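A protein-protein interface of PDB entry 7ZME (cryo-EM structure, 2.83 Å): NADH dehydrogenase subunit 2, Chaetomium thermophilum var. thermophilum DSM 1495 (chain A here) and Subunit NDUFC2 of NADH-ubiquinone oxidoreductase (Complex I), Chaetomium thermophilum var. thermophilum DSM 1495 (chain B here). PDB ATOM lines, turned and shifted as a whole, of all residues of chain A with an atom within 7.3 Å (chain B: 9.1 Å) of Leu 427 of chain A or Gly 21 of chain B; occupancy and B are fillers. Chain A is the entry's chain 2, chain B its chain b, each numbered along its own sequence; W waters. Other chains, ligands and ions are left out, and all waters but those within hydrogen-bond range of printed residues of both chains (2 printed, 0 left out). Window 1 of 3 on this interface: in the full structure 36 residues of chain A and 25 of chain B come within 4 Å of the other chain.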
ATOM      1  N   TYR A 421      12.738 -12.885 -30.949  1.00  0.00           N
ATOM      2  CA  TYR A 421      13.596 -13.637 -30.006  1.00  0.00           C
ATOM      3  C   TYR A 421      13.050 -15.053 -29.872  1.00  0.00           C
ATOM      4  O   TYR A 421      13.771 -15.928 -29.390  1.00  0.00           O
ATOM      5  CB  TYR A 421      13.829 -12.886 -28.692  1.00  0.00           C
ATOM      6  CG  TYR A 421      14.895 -13.539 -27.851  1.00  0.00           C
ATOM      7  CD1 TYR A 421      16.233 -13.428 -28.187  1.00  0.00           C
ATOM      8  CD2 TYR A 421      14.564 -14.329 -26.764  1.00  0.00           C
ATOM      9  CE1 TYR A 421      17.218 -14.055 -27.444  1.00  0.00           C
ATOM     10  CE2 TYR A 421      15.534 -14.972 -26.016  1.00  0.00           C
ATOM     11  CZ  TYR A 421      16.866 -14.827 -26.353  1.00  0.00           C
ATOM     12  OH  TYR A 421      17.823 -15.447 -25.609  1.00  0.00           O
ATOM     13  N   PHE A 422      11.820 -15.258 -30.335  1.00  0.00           N
ATOM     14  CA  PHE A 422      11.192 -16.597 -30.295  1.00  0.00           C
ATOM     15  C   PHE A 422      11.922 -17.495 -31.288  1.00  0.00           C
ATOM     16  O   PHE A 422      11.964 -18.715 -31.096  1.00  0.00           O
ATOM     17  CB  PHE A 422       9.697 -16.455 -30.586  1.00  0.00           C
ATOM     18  CG  PHE A 422       8.974 -17.738 -30.899  1.00  0.00           C
ATOM     19  CD1 PHE A 422       8.672 -18.644 -29.896  1.00  0.00           C
ATOM     20  CD2 PHE A 422       8.591 -18.035 -32.197  1.00  0.00           C
ATOM     21  CE1 PHE A 422       8.010 -19.824 -30.184  1.00  0.00           C
ATOM     22  CE2 PHE A 422       7.930 -19.218 -32.484  1.00  0.00           C
ATOM     23  CZ  PHE A 422       7.641 -20.107 -31.477  1.00  0.00           C
ATOM     24  N   ILE A 424      15.138 -17.182 -31.907  1.00  0.00           N
ATOM     25  CA  ILE A 424      16.520 -17.399 -31.389  1.00  0.00           C
ATOM     26  C   ILE A 424      16.472 -18.330 -30.173  1.00  0.00           C
ATOM     27  O   ILE A 424      17.138 -19.367 -30.224  1.00  0.00           O
ATOM     28  CB  ILE A 424      17.187 -16.043 -31.082  1.00  0.00           C
ATOM     29  CG1 ILE A 424      17.374 -15.211 -32.352  1.00  0.00           C
ATOM     30  CG2 ILE A 424      18.492 -16.224 -30.325  1.00  0.00           C
ATOM     31  CD1 ILE A 424      17.932 -13.836 -32.100  1.00  0.00           C
ATOM     32  N   ASN A 425      15.670 -18.005 -29.154  1.00  0.00           N
ATOM     33  CA  ASN A 425      15.489 -18.898 -27.978  1.00  0.00           C
ATOM     34  C   ASN A 425      13.987 -19.010 -27.718  1.00  0.00           C
ATOM     35  O   ASN A 425      13.485 -18.167 -26.972  1.00  0.00           O
ATOM     36  CB  ASN A 425      16.213 -18.446 -26.715  1.00  0.00           C
ATOM     37  CG  ASN A 425      16.384 -19.550 -25.694  1.00  0.00           C
ATOM     38  OD1 ASN A 425      15.474 -20.337 -25.457  1.00  0.00           O
ATOM     39  ND2 ASN A 425      17.547 -19.604 -25.072  1.00  0.00           N
ATOM     40  N   PRO A 426      13.260 -20.025 -28.246  1.00  0.00           N
ATOM     41  CA  PRO A 426      11.799 -20.066 -28.118  1.00  0.00           C
ATOM     42  C   PRO A 426      11.261 -20.192 -26.687  1.00  0.00           C
ATOM     43  O   PRO A 426      10.328 -19.511 -26.370  1.00  0.00           O
ATOM     44  CB  PRO A 426      11.399 -21.312 -28.925  1.00  0.00           C
ATOM     45  CG  PRO A 426      12.642 -22.161 -28.966  1.00  0.00           C
ATOM     46  CD  PRO A 426      13.791 -21.179 -28.969  1.00  0.00           C
ATOM     47  N   LEU A 427      11.854 -21.058 -25.872  1.00  0.00           N
ATOM     48  CA  LEU A 427      11.323 -21.294 -24.536  1.00  0.00           C
ATOM     49  C   LEU A 427      11.689 -20.179 -23.568  1.00  0.00           C
ATOM     50  O   LEU A 427      10.918 -19.886 -22.648  1.00  0.00           O
ATOM     51  CB  LEU A 427      11.796 -22.643 -23.998  1.00  0.00           C
ATOM     52  CG  LEU A 427      10.909 -23.181 -22.874  1.00  0.00           C
ATOM     53  CD1 LEU A 427       9.443 -23.006 -23.240  1.00  0.00           C
ATOM     54  CD2 LEU A 427      11.214 -24.636 -22.555  1.00  0.00           C
ATOM     55  N   LEU A 428      12.847 -19.548 -23.750  1.00  0.00           N
ATOM     56  CA  LEU A 428      13.159 -18.361 -22.968  1.00  0.00           C
ATOM     57  C   LEU A 428      12.231 -17.209 -23.325  1.00  0.00           C
ATOM     58  O   LEU A 428      11.939 -16.358 -22.479  1.00  0.00           O
ATOM     59  CB  LEU A 428      14.622 -17.971 -23.177  1.00  0.00           C
ATOM     60  CG  LEU A 428      15.198 -16.817 -22.362  1.00  0.00           C
ATOM     61  CD1 LEU A 428      14.947 -17.022 -20.881  1.00  0.00           C
ATOM     62  CD2 LEU A 428      16.678 -16.663 -22.643  1.00  0.00           C
ATOM     63  N   SER A 429      11.750 -17.173 -24.568  1.00  0.00           N
ATOM     64  CA  SER A 429      10.797 -16.147 -24.971  1.00  0.00           C
ATOM     65  C   SER A 429       9.419 -16.408 -24.382  1.00  0.00           C
ATOM     66  O   SER A 429       8.706 -15.469 -24.015  1.00  0.00           O
ATOM     67  CB  SER A 429      10.724 -16.083 -26.493  1.00  0.00           C
ATOM     68  OG  SER A 429      12.017 -16.117 -27.053  1.00  0.00           O
ATOM     69  N   LEU A 430       9.020 -17.678 -24.304  1.00  0.00           N
ATOM     70  CA  LEU A 430       7.755 -18.020 -23.671  1.00  0.00           C
ATOM     71  C   LEU A 430       7.802 -17.789 -22.168  1.00  0.00           C
ATOM     72  O   LEU A 430       6.771 -17.497 -21.555  1.00  0.00           O
ATOM     73  CB  LEU A 430       7.397 -19.471 -23.980  1.00  0.00           C
ATOM     74  CG  LEU A 430       5.986 -19.921 -23.612  1.00  0.00           C
ATOM     75  CD1 LEU A 430       4.982 -19.402 -24.619  1.00  0.00           C
ATOM     76  CD2 LEU A 430       5.927 -21.425 -23.525  1.00  0.00           C
ATOM     77  N   SER A 431       8.982 -17.918 -21.559  1.00  0.00           N
ATOM     78  CA  SER A 431       9.132 -17.555 -20.155  1.00  0.00           C
ATOM     79  C   SER A 431       8.832 -16.080 -19.939  1.00  0.00           C
ATOM     80  O   SER A 431       8.140 -15.713 -18.984  1.00  0.00           O
ATOM     81  CB  SER A 431      10.547 -17.881 -19.681  1.00  0.00           C
ATOM     82  OG  SER A 431      10.801 -19.267 -19.752  1.00  0.00           O
ATOM     83  N   LEU A 432       9.349 -15.219 -20.818  1.00  0.00           N
ATOM     84  CA  LEU A 432       9.065 -13.795 -20.723  1.00  0.00           C
ATOM     85  C   LEU A 432       7.607 -13.501 -21.049  1.00  0.00           C
ATOM     86  O   LEU A 432       6.998 -12.612 -20.444  1.00  0.00           O
ATOM     87  CB  LEU A 432       9.995 -13.016 -21.649  1.00  0.00           C
ATOM     88  CG  LEU A 432       9.954 -11.492 -21.557  1.00  0.00           C
ATOM     89  CD1 LEU A 432      10.081 -11.021 -20.118  1.00  0.00           C
ATOM     90  CD2 LEU A 432      11.046 -10.896 -22.413  1.00  0.00           C
ATOM     91  N   ALA A 433       7.029 -14.239 -21.998  1.00  0.00           N
ATOM     92  CA  ALA A 433       5.622 -14.045 -22.330  1.00  0.00           C
ATOM     93  C   ALA A 433       4.723 -14.355 -21.140  1.00  0.00           C
ATOM     94  O   ALA A 433       3.764 -13.624 -20.873  1.00  0.00           O
ATOM     95  CB  ALA A 433       5.241 -14.910 -23.531  1.00  0.00           C
ATOM     96  N   ILE A 434       5.019 -15.431 -20.412  1.00  0.00           N
ATOM     97  CA  ILE A 434       4.222 -15.783 -19.243  1.00  0.00           C
ATOM     98  C   ILE A 434       4.367 -14.724 -18.155  1.00  0.00           C
ATOM     99  O   ILE A 434       3.387 -14.349 -17.498  1.00  0.00           O
ATOM    100  CB  ILE A 434       4.614 -17.187 -18.745  1.00  0.00           C
ATOM    101  CG1 ILE A 434       4.092 -18.251 -19.711  1.00  0.00           C
ATOM    102  CG2 ILE A 434       4.086 -17.441 -17.347  1.00  0.00           C
ATOM    103  CD1 ILE A 434       4.733 -19.600 -19.546  1.00  0.00           C
ATOM    104  N   ILE A 532      23.804 -20.811 -21.577  1.00  0.00           N
ATOM    105  CA  ILE A 532      23.587 -19.984 -20.360  1.00  0.00           C
ATOM    106  C   ILE A 532      23.994 -20.848 -19.168  1.00  0.00           C
ATOM    107  O   ILE A 532      23.695 -22.047 -19.201  1.00  0.00           O
ATOM    108  CB  ILE A 532      22.094 -19.633 -20.286  1.00  0.00           C
ATOM    109  CG1 ILE A 532      21.634 -18.859 -21.524  1.00  0.00           C
ATOM    110  CG2 ILE A 532      21.762 -18.902 -18.997  1.00  0.00           C
ATOM    111  CD1 ILE A 532      20.169 -19.039 -21.856  1.00  0.00           C
ATOM    112  N   SER A 537      19.254 -20.345 -15.646  1.00  0.00           N
ATOM    113  CA  SER A 537      18.179 -21.084 -16.297  1.00  0.00           C
ATOM    114  C   SER A 537      17.286 -21.785 -15.280  1.00  0.00           C
ATOM    115  O   SER A 537      16.066 -21.832 -15.460  1.00  0.00           O
ATOM    116  CB  SER A 537      18.753 -22.089 -17.294  1.00  0.00           C
ATOM    117  OG  SER A 537      19.856 -22.780 -16.744  1.00  0.00           O
ATOM    118  N   ILE A 540      15.018 -19.013 -13.619  1.00  0.00           N
ATOM    119  CA  ILE A 540      13.926 -18.607 -14.496  1.00  0.00           C
ATOM    120  C   ILE A 540      12.916 -19.735 -14.639  1.00  0.00           C
ATOM    121  O   ILE A 540      11.704 -19.502 -14.684  1.00  0.00           O
ATOM    122  CB  ILE A 540      14.471 -18.155 -15.862  1.00  0.00           C
ATOM    123  CG1 ILE A 540      15.362 -16.926 -15.698  1.00  0.00           C
ATOM    124  CG2 ILE A 540      13.330 -17.846 -16.811  1.00  0.00           C
ATOM    125  CD1 ILE A 540      15.946 -16.417 -16.988  1.00  0.00           C
ATOM    126  N   THR A 544       9.011 -19.146 -13.553  1.00  0.00           N
ATOM    127  CA  THR A 544       8.026 -19.325 -14.614  1.00  0.00           C
ATOM    128  C   THR A 544       7.006 -20.390 -14.232  1.00  0.00           C
ATOM    129  O   THR A 544       5.801 -20.216 -14.451  1.00  0.00           O
ATOM    130  CB  THR A 544       8.720 -19.694 -15.926  1.00  0.00           C
ATOM    131  OG1 THR A 544       9.818 -18.805 -16.149  1.00  0.00           O
ATOM    132  CG2 THR A 544       7.754 -19.590 -17.096  1.00  0.00           C
ATOM    133  N   ALA B  14       9.272 -30.726 -14.390  1.00  0.00           N
ATOM    134  CA  ALA B  14       9.043 -29.664 -15.360  1.00  0.00           C
ATOM    135  C   ALA B  14      10.082 -28.559 -15.241  1.00  0.00           C
ATOM    136  O   ALA B  14      10.373 -27.879 -16.229  1.00  0.00           O
ATOM    137  CB  ALA B  14       7.638 -29.092 -15.192  1.00  0.00           C
ATOM    138  N   VAL B  15      10.639 -28.351 -14.048  1.00  0.00           N
ATOM    139  CA  VAL B  15      11.716 -27.381 -13.908  1.00  0.00           C
ATOM    140  C   VAL B  15      12.940 -27.839 -14.687  1.00  0.00           C
ATOM    141  O   VAL B  15      13.573 -27.050 -15.395  1.00  0.00           O
ATOM    142  CB  VAL B  15      12.039 -27.145 -12.422  1.00  0.00           C
ATOM    143  CG1 VAL B  15      13.285 -26.284 -12.279  1.00  0.00           C
ATOM    144  CG2 VAL B  15      10.861 -26.494 -11.720  1.00  0.00           C
ATOM    145  N   ARG B  16      13.285 -29.122 -14.579  1.00  0.00           N
ATOM    146  CA  ARG B  16      14.391 -29.663 -15.360  1.00  0.00           C
ATOM    147  C   ARG B  16      14.096 -29.597 -16.852  1.00  0.00           C
ATOM    148  O   ARG B  16      14.983 -29.291 -17.654  1.00  0.00           O
ATOM    149  CB  ARG B  16      14.678 -31.097 -14.925  1.00  0.00           C
ATOM    150  CG  ARG B  16      15.914 -31.708 -15.543  1.00  0.00           C
ATOM    151  CD  ARG B  16      17.117 -30.812 -15.414  1.00  0.00           C
ATOM    152  NE  ARG B  16      18.279 -31.425 -16.038  1.00  0.00           N
ATOM    153  CZ  ARG B  16      19.502 -30.914 -16.011  1.00  0.00           C
ATOM    154  NH1 ARG B  16      20.495 -31.549 -16.610  1.00  0.00           N
ATOM    155  NH2 ARG B  16      19.728 -29.768 -15.393  1.00  0.00           N
ATOM    156  N   PHE B  17      12.854 -29.886 -17.241  1.00  0.00           N
ATOM    157  CA  PHE B  17      12.469 -29.778 -18.644  1.00  0.00           C
ATOM    158  C   PHE B  17      12.566 -28.339 -19.131  1.00  0.00           C
ATOM    159  O   PHE B  17      13.174 -28.061 -20.170  1.00  0.00           O
ATOM    160  CB  PHE B  17      11.051 -30.309 -18.836  1.00  0.00           C
ATOM    161  CG  PHE B  17      10.747 -30.717 -20.242  1.00  0.00           C
ATOM    162  CD1 PHE B  17      11.378 -31.807 -20.812  1.00  0.00           C
ATOM    163  CD2 PHE B  17       9.837 -30.002 -20.999  1.00  0.00           C
ATOM    164  CE1 PHE B  17      11.100 -32.183 -22.108  1.00  0.00           C
ATOM    165  CE2 PHE B  17       9.554 -30.370 -22.292  1.00  0.00           C
ATOM    166  CZ  PHE B  17      10.187 -31.463 -22.850  1.00  0.00           C
ATOM    167  N   TRP B  18      11.967 -27.409 -18.389  1.00  0.00           N
ATOM    168  CA  TRP B  18      11.974 -26.014 -18.811  1.00  0.00           C
ATOM    169  C   TRP B  18      13.377 -25.431 -18.792  1.00  0.00           C
ATOM    170  O   TRP B  18      13.681 -24.522 -19.569  1.00  0.00           O
ATOM    171  CB  TRP B  18      11.051 -25.194 -17.917  1.00  0.00           C
ATOM    172  CG  TRP B  18       9.695 -24.998 -18.484  1.00  0.00           C
ATOM    173  CD1 TRP B  18       8.691 -25.916 -18.535  1.00  0.00           C
ATOM    174  CD2 TRP B  18       9.183 -23.810 -19.090  1.00  0.00           C
ATOM    175  NE1 TRP B  18       7.581 -25.372 -19.131  1.00  0.00           N
ATOM    176  CE2 TRP B  18       7.860 -24.078 -19.482  1.00  0.00           C
ATOM    177  CE3 TRP B  18       9.715 -22.545 -19.341  1.00  0.00           C
ATOM    178  CZ2 TRP B  18       7.063 -23.129 -20.113  1.00  0.00           C
ATOM    179  CZ3 TRP B  18       8.921 -21.609 -19.963  1.00  0.00           C
ATOM    180  CH2 TRP B  18       7.611 -21.903 -20.342  1.00  0.00           C
ATOM    181  N   GLN B  19      14.240 -25.940 -17.915  1.00  0.00           N
ATOM    182  CA  GLN B  19      15.588 -25.403 -17.794  1.00  0.00           C
ATOM    183  C   GLN B  19      16.441 -25.777 -18.996  1.00  0.00           C
ATOM    184  O   GLN B  19      17.219 -24.955 -19.493  1.00  0.00           O
ATOM    185  CB  GLN B  19      16.211 -25.894 -16.489  1.00  0.00           C
ATOM    186  CG  GLN B  19      17.508 -25.246 -16.112  1.00  0.00           C
ATOM    187  CD  GLN B  19      18.680 -26.184 -16.212  1.00  0.00           C
ATOM    188  OE1 GLN B  19      18.542 -27.384 -16.005  1.00  0.00           O
ATOM    189  NE2 GLN B  19      19.849 -25.640 -16.501  1.00  0.00           N
ATOM    190  N   LEU B  20      16.304 -27.009 -19.484  1.00  0.00           N
ATOM    191  CA  LEU B  20      17.039 -27.416 -20.675  1.00  0.00           C
ATOM    192  C   LEU B  20      16.507 -26.726 -21.921  1.00  0.00           C
ATOM    193  O   LEU B  20      17.276 -26.437 -22.843  1.00  0.00           O
ATOM    194  CB  LEU B  20      16.984 -28.934 -20.831  1.00  0.00           C
ATOM    195  CG  LEU B  20      17.495 -29.725 -19.624  1.00  0.00           C
ATOM    196  CD1 LEU B  20      17.387 -31.219 -19.857  1.00  0.00           C
ATOM    197  CD2 LEU B  20      18.924 -29.332 -19.298  1.00  0.00           C
ATOM    198  N   GLY B  21      15.212 -26.435 -21.946  1.00  0.00           N
ATOM    199  CA  GLY B  21      14.644 -25.690 -23.079  1.00  0.00           C
ATOM    200  C   GLY B  21      15.212 -24.293 -23.136  1.00  0.00           C
ATOM    201  O   GLY B  21      15.645 -23.886 -24.222  1.00  0.00           O
ATOM    202  N   ILE B  22      15.202 -23.574 -22.015  1.00  0.00           N
ATOM    203  CA  ILE B  22      15.733 -22.181 -21.971  1.00  0.00           C
ATOM    204  C   ILE B  22      17.204 -22.197 -22.384  1.00  0.00           C
ATOM    205  O   ILE B  22      17.627 -21.248 -23.049  1.00  0.00           O
ATOM    206  CB  ILE B  22      15.559 -21.556 -20.578  1.00  0.00           C
ATOM    207  CG1 ILE B  22      14.133 -21.049 -20.348  1.00  0.00           C
ATOM    208  CG2 ILE B  22      16.590 -20.463 -20.344  1.00  0.00           C
ATOM    209  CD1 ILE B  22      13.814 -20.786 -18.899  1.00  0.00           C
ATOM    210  N   GLU B  23      17.958 -23.216 -21.985  1.00  0.00           N
ATOM    211  CA  GLU B  23      19.400 -23.304 -22.312  1.00  0.00           C
ATOM    212  C   GLU B  23      19.553 -23.851 -23.724  1.00  0.00           C
ATOM    213  O   GLU B  23      20.689 -23.869 -24.225  1.00  0.00           O
ATOM    214  CB  GLU B  23      20.098 -24.228 -21.319  1.00  0.00           C
ATOM    215  CG  GLU B  23      20.620 -23.516 -20.093  1.00  0.00           C
ATOM    216  CD  GLU B  23      21.258 -24.457 -19.089  1.00  0.00           C
ATOM    217  OE1 GLU B  23      21.914 -23.965 -18.158  1.00  0.00           O
ATOM    218  OE2 GLU B  23      21.086 -25.680 -19.239  1.00  0.00           O
ATOM    219  N   MET B  24      18.455 -24.294 -24.330  1.00  0.00           N
ATOM    220  CA  MET B  24      18.485 -24.902 -25.685  1.00  0.00           C
ATOM    221  C   MET B  24      19.414 -26.110 -25.671  1.00  0.00           C
ATOM    222  O   MET B  24      20.125 -26.322 -26.660  1.00  0.00           O
ATOM    223  CB  MET B  24      18.817 -23.891 -26.780  1.00  0.00           C
ATOM    224  CG  MET B  24      17.729 -22.852 -26.936  1.00  0.00           C
ATOM    225  SD  MET B  24      17.891 -21.815 -28.399  1.00  0.00           S
ATOM    226  CE  MET B  24      19.455 -21.007 -28.068  1.00  0.00           C
ATOM    227  N   ARG B  25      19.372 -26.879 -24.585  1.00  0.00           N
ATOM    228  CA  ARG B  25      20.157 -28.129 -24.497  1.00  0.00           C
ATOM    229  C   ARG B  25      19.181 -29.300 -24.680  1.00  0.00           C
ATOM    230  O   ARG B  25      18.060 -29.181 -24.180  1.00  0.00           O
ATOM    231  CB  ARG B  25      20.862 -28.250 -23.143  1.00  0.00           C
ATOM    232  CG  ARG B  25      22.235 -27.605 -23.068  1.00  0.00           C
ATOM    233  CD  ARG B  25      22.693 -27.630 -21.625  1.00  0.00           C
ATOM    234  NE  ARG B  25      22.449 -28.934 -21.026  1.00  0.00           N
ATOM    235  CZ  ARG B  25      22.520 -29.193 -19.727  1.00  0.00           C
ATOM    236  NH1 ARG B  25      22.282 -30.413 -19.283  1.00  0.00           N
ATOM    237  NH2 ARG B  25      22.818 -28.231 -18.872  1.00  0.00           N
ATOM    238  N   PRO B  26      19.536 -30.438 -25.321  1.00  0.00           N
ATOM    239  CA  PRO B  26      18.576 -31.514 -25.594  1.00  0.00           C
ATOM    240  C   PRO B  26      18.043 -32.123 -24.304  1.00  0.00           C
ATOM    241  O   PRO B  26      18.797 -32.391 -23.366  1.00  0.00           O
ATOM    242  CB  PRO B  26      19.398 -32.525 -26.401  1.00  0.00           C
ATOM    243  CG  PRO B  26      20.817 -32.232 -26.041  1.00  0.00           C
ATOM    244  CD  PRO B  26      20.890 -30.763 -25.801  1.00  0.00           C
ATOM    245  N   PHE B  27      16.731 -32.328 -24.255  1.00  0.00           N
ATOM    246  CA  PHE B  27      16.162 -33.097 -23.163  1.00  0.00           C
ATOM    247  C   PHE B  27      16.583 -34.554 -23.294  1.00  0.00           C
ATOM    248  O   PHE B  27      16.735 -35.082 -24.397  1.00  0.00           O
ATOM    249  CB  PHE B  27      14.636 -33.024 -23.150  1.00  0.00           C
ATOM    250  CG  PHE B  27      14.072 -31.689 -23.532  1.00  0.00           C
ATOM    251  CD1 PHE B  27      14.149 -30.613 -22.671  1.00  0.00           C
ATOM    252  CD2 PHE B  27      13.421 -31.526 -24.738  1.00  0.00           C
ATOM    253  CE1 PHE B  27      13.611 -29.393 -23.020  1.00  0.00           C
ATOM    254  CE2 PHE B  27      12.884 -30.310 -25.089  1.00  0.00           C
ATOM    255  CZ  PHE B  27      12.977 -29.244 -24.227  1.00  0.00           C
ATOM    256  N   PHE B  28      16.784 -35.197 -22.149  1.00  0.00           N
ATOM    257  CA  PHE B  28      17.028 -36.637 -22.093  1.00  0.00           C
ATOM    258  C   PHE B  28      18.322 -37.027 -22.796  1.00  0.00           C
ATOM    259  O   PHE B  28      18.358 -37.961 -23.597  1.00  0.00           O
ATOM    260  CB  PHE B  28      15.841 -37.418 -22.656  1.00  0.00           C
ATOM    261  CG  PHE B  28      14.518 -36.904 -22.192  1.00  0.00           C
ATOM    262  CD1 PHE B  28      14.259 -36.756 -20.843  1.00  0.00           C
ATOM    263  CD2 PHE B  28      13.538 -36.555 -23.096  1.00  0.00           C
ATOM    264  CE1 PHE B  28      13.047 -36.278 -20.406  1.00  0.00           C
ATOM    265  CE2 PHE B  28      12.327 -36.080 -22.657  1.00  0.00           C
ATOM    266  CZ  PHE B  28      12.081 -35.942 -21.312  1.00  0.00           C
ATOM    267  N   TYR B  36      16.791 -35.803 -13.551  1.00  0.00           N
ATOM    268  CA  TYR B  36      15.342 -35.857 -13.409  1.00  0.00           C
ATOM    269  C   TYR B  36      14.962 -36.511 -12.082  1.00  0.00           C
ATOM    270  O   TYR B  36      14.050 -36.023 -11.405  1.00  0.00           O
ATOM    271  CB  TYR B  36      14.701 -36.571 -14.602  1.00  0.00           C
ATOM    272  CG  TYR B  36      14.640 -35.711 -15.842  1.00  0.00           C
ATOM    273  CD1 TYR B  36      13.654 -34.752 -15.995  1.00  0.00           C
ATOM    274  CD2 TYR B  36      15.580 -35.846 -16.849  1.00  0.00           C
ATOM    275  CE1 TYR B  36      13.601 -33.960 -17.118  1.00  0.00           C
ATOM    276  CE2 TYR B  36      15.533 -35.061 -17.974  1.00  0.00           C
ATOM    277  CZ  TYR B  36      14.543 -34.117 -18.104  1.00  0.00           C
ATOM    278  OH  TYR B  36      14.494 -33.329 -19.227  1.00  0.00           O
HETATM  279  O   HOH W   1      14.341 -22.626 -26.128  1.00  0.00           O
HETATM  280  O   HOH W   2      21.865 -21.182 -23.940  1.00  0.00           O
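Water W1 lies within hydrogen-bond range of O of Gly 21 of chain B, OD1 of Asn 425 of chain A and N of Leu 427 of chain A. Water W2 lies within hydrogen-bond range of O of Glu 23 of chain B (2.9 Å) and N of Ile 532 of chain A (3.1 Å).
NE2 of Gln 19 of chain B is in hydrogen-bond range of OE2 of Glu 23 of chain B. The backbone carbonyl oxygen (O) of Ile 540 of chain A lies within hydrogen-bond range of the side-chain hydroxyl (OG1) of Thr 544 of chain A (2.5 Å). The side-chain carboxylate of Glu 23 of chain B is in salt-bridge range of the guanidinium group of Arg 25 of chain B (3.1 Å). The guanidinium group (NH2) of Arg 16 of chain B sits at hydrogen-bond distance from the side-chain amide oxygen (OE1) of Gln 19 of chain B (2.7 Å). O of Asn 425 of chain A lies within hydrogen-bond range of OG of Ser 429 of chain A (2.5 Å). The side-chain amide oxygen (OD1) of Asn 425 of chain A lies within hydrogen-bond range of the backbone NH (N) of Leu 428 of chain A (3.2 Å).
Of the printed residues of chain B, Leu 427 of chain A touches Trp 18 (3.6 Å) and Gly 21 (3.6 Å). Of chain A, only Asn 425 and Leu 427 come within 4 Å of Gly 21 of chain B. Printed residues of chain B within 4 Å of Leu 428 of chain A: Ile 22 (3.9 Å). Of the printed residues of chain B, Ile 540 of chain A touches Ile 22 (3.6 Å). Printed residues of chain A within 4 Å of Glu 23 of chain B: Ile 532 and Ser 537. Of the printed residues of chain B, Asn 425 of chain A touches Gly 21 (3.8 Å), Ile 22 (2.6 Å) and Met 24 (3.7 Å). Of the printed residues of chain A, Met 24 of chain B touches Ile 424 (3.1 Å) and Asn 425 (3.7 Å). Ser 429 of chain A touches none of the printed residues of chain B. Phe 28 of chain B touches none of the printed residues of chain A. The nearest residue of chain A that does not touch Gly 21 of chain B is Leu 428 of chain A (5.2 Å).
Asn 425 of chain A touches Gly 21 of chain B (OD1 to O, 3.8 Å). CG of Met 24 of chain B touches OD1 of Asn 425 of chain A (3.7 Å). CD1 of Leu 427 of chain A touches CZ3 of Trp 18 of chain B (3.6 Å). Leu 427 of chain A touches Gly 21 of chain B (CD2 to CA, 3.6 Å). Ser 431 of chain A touches Trp 18 of chain B (OG to CZ3, 3.0 Å). OG of Ser 431 of chain A touches CD1 of Ile 22 of chain B, 3.5 Å away. Ile 434 of chain A touches Trp 18 of chain B (CD1 to CH2, 3.8 Å). Ile 532 of chain A touches Ile 22 of chain B. Ile 22 of chain B touches Ile 540 of chain A (CD1 to CG2, 3.6 Å). CZ3 of Trp 18 of chain B touches CG2 of Thr 544 of chain A, at 3.7 Å.
Of the 16 printed residues of chain B, 6 touch a printed residue of chain A. Hydrophobic or aromatic side chains of chain B that line the printed part of chain A: Trp 18, Ile 22 and Met 24. Among the printed residues, 17 pairs touch across the chains. Among the printed residues, no Asp or Glu carboxylate lies within 4 Å of a Lys or Arg side-chain nitrogen of the other chain.
NE2 of Gln 19 of chain B lies within hydrogen-bond range of OG of Ser 537 of chain A (2.9 Å). The backbone carbonyl oxygen of Ile 532 of chain A sits close to the side-chain carboxylate of Glu 23 of chain B (2.8 Å). The backbone carbonyl oxygen of Ile 22 of chain B is in hydrogen-bond range of the side-chain amide nitrogen of Asn 425 of chain A. The side-chain hydroxyl (OG) of Ser 537 of chain A sits at hydrogen-bond distance from the side-chain carboxylate (OE1) of Glu 23 of chain B (2.8 Å). O of Ile 424 of chain A lies close to SD of Met 24 of chain B (3.1 Å).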
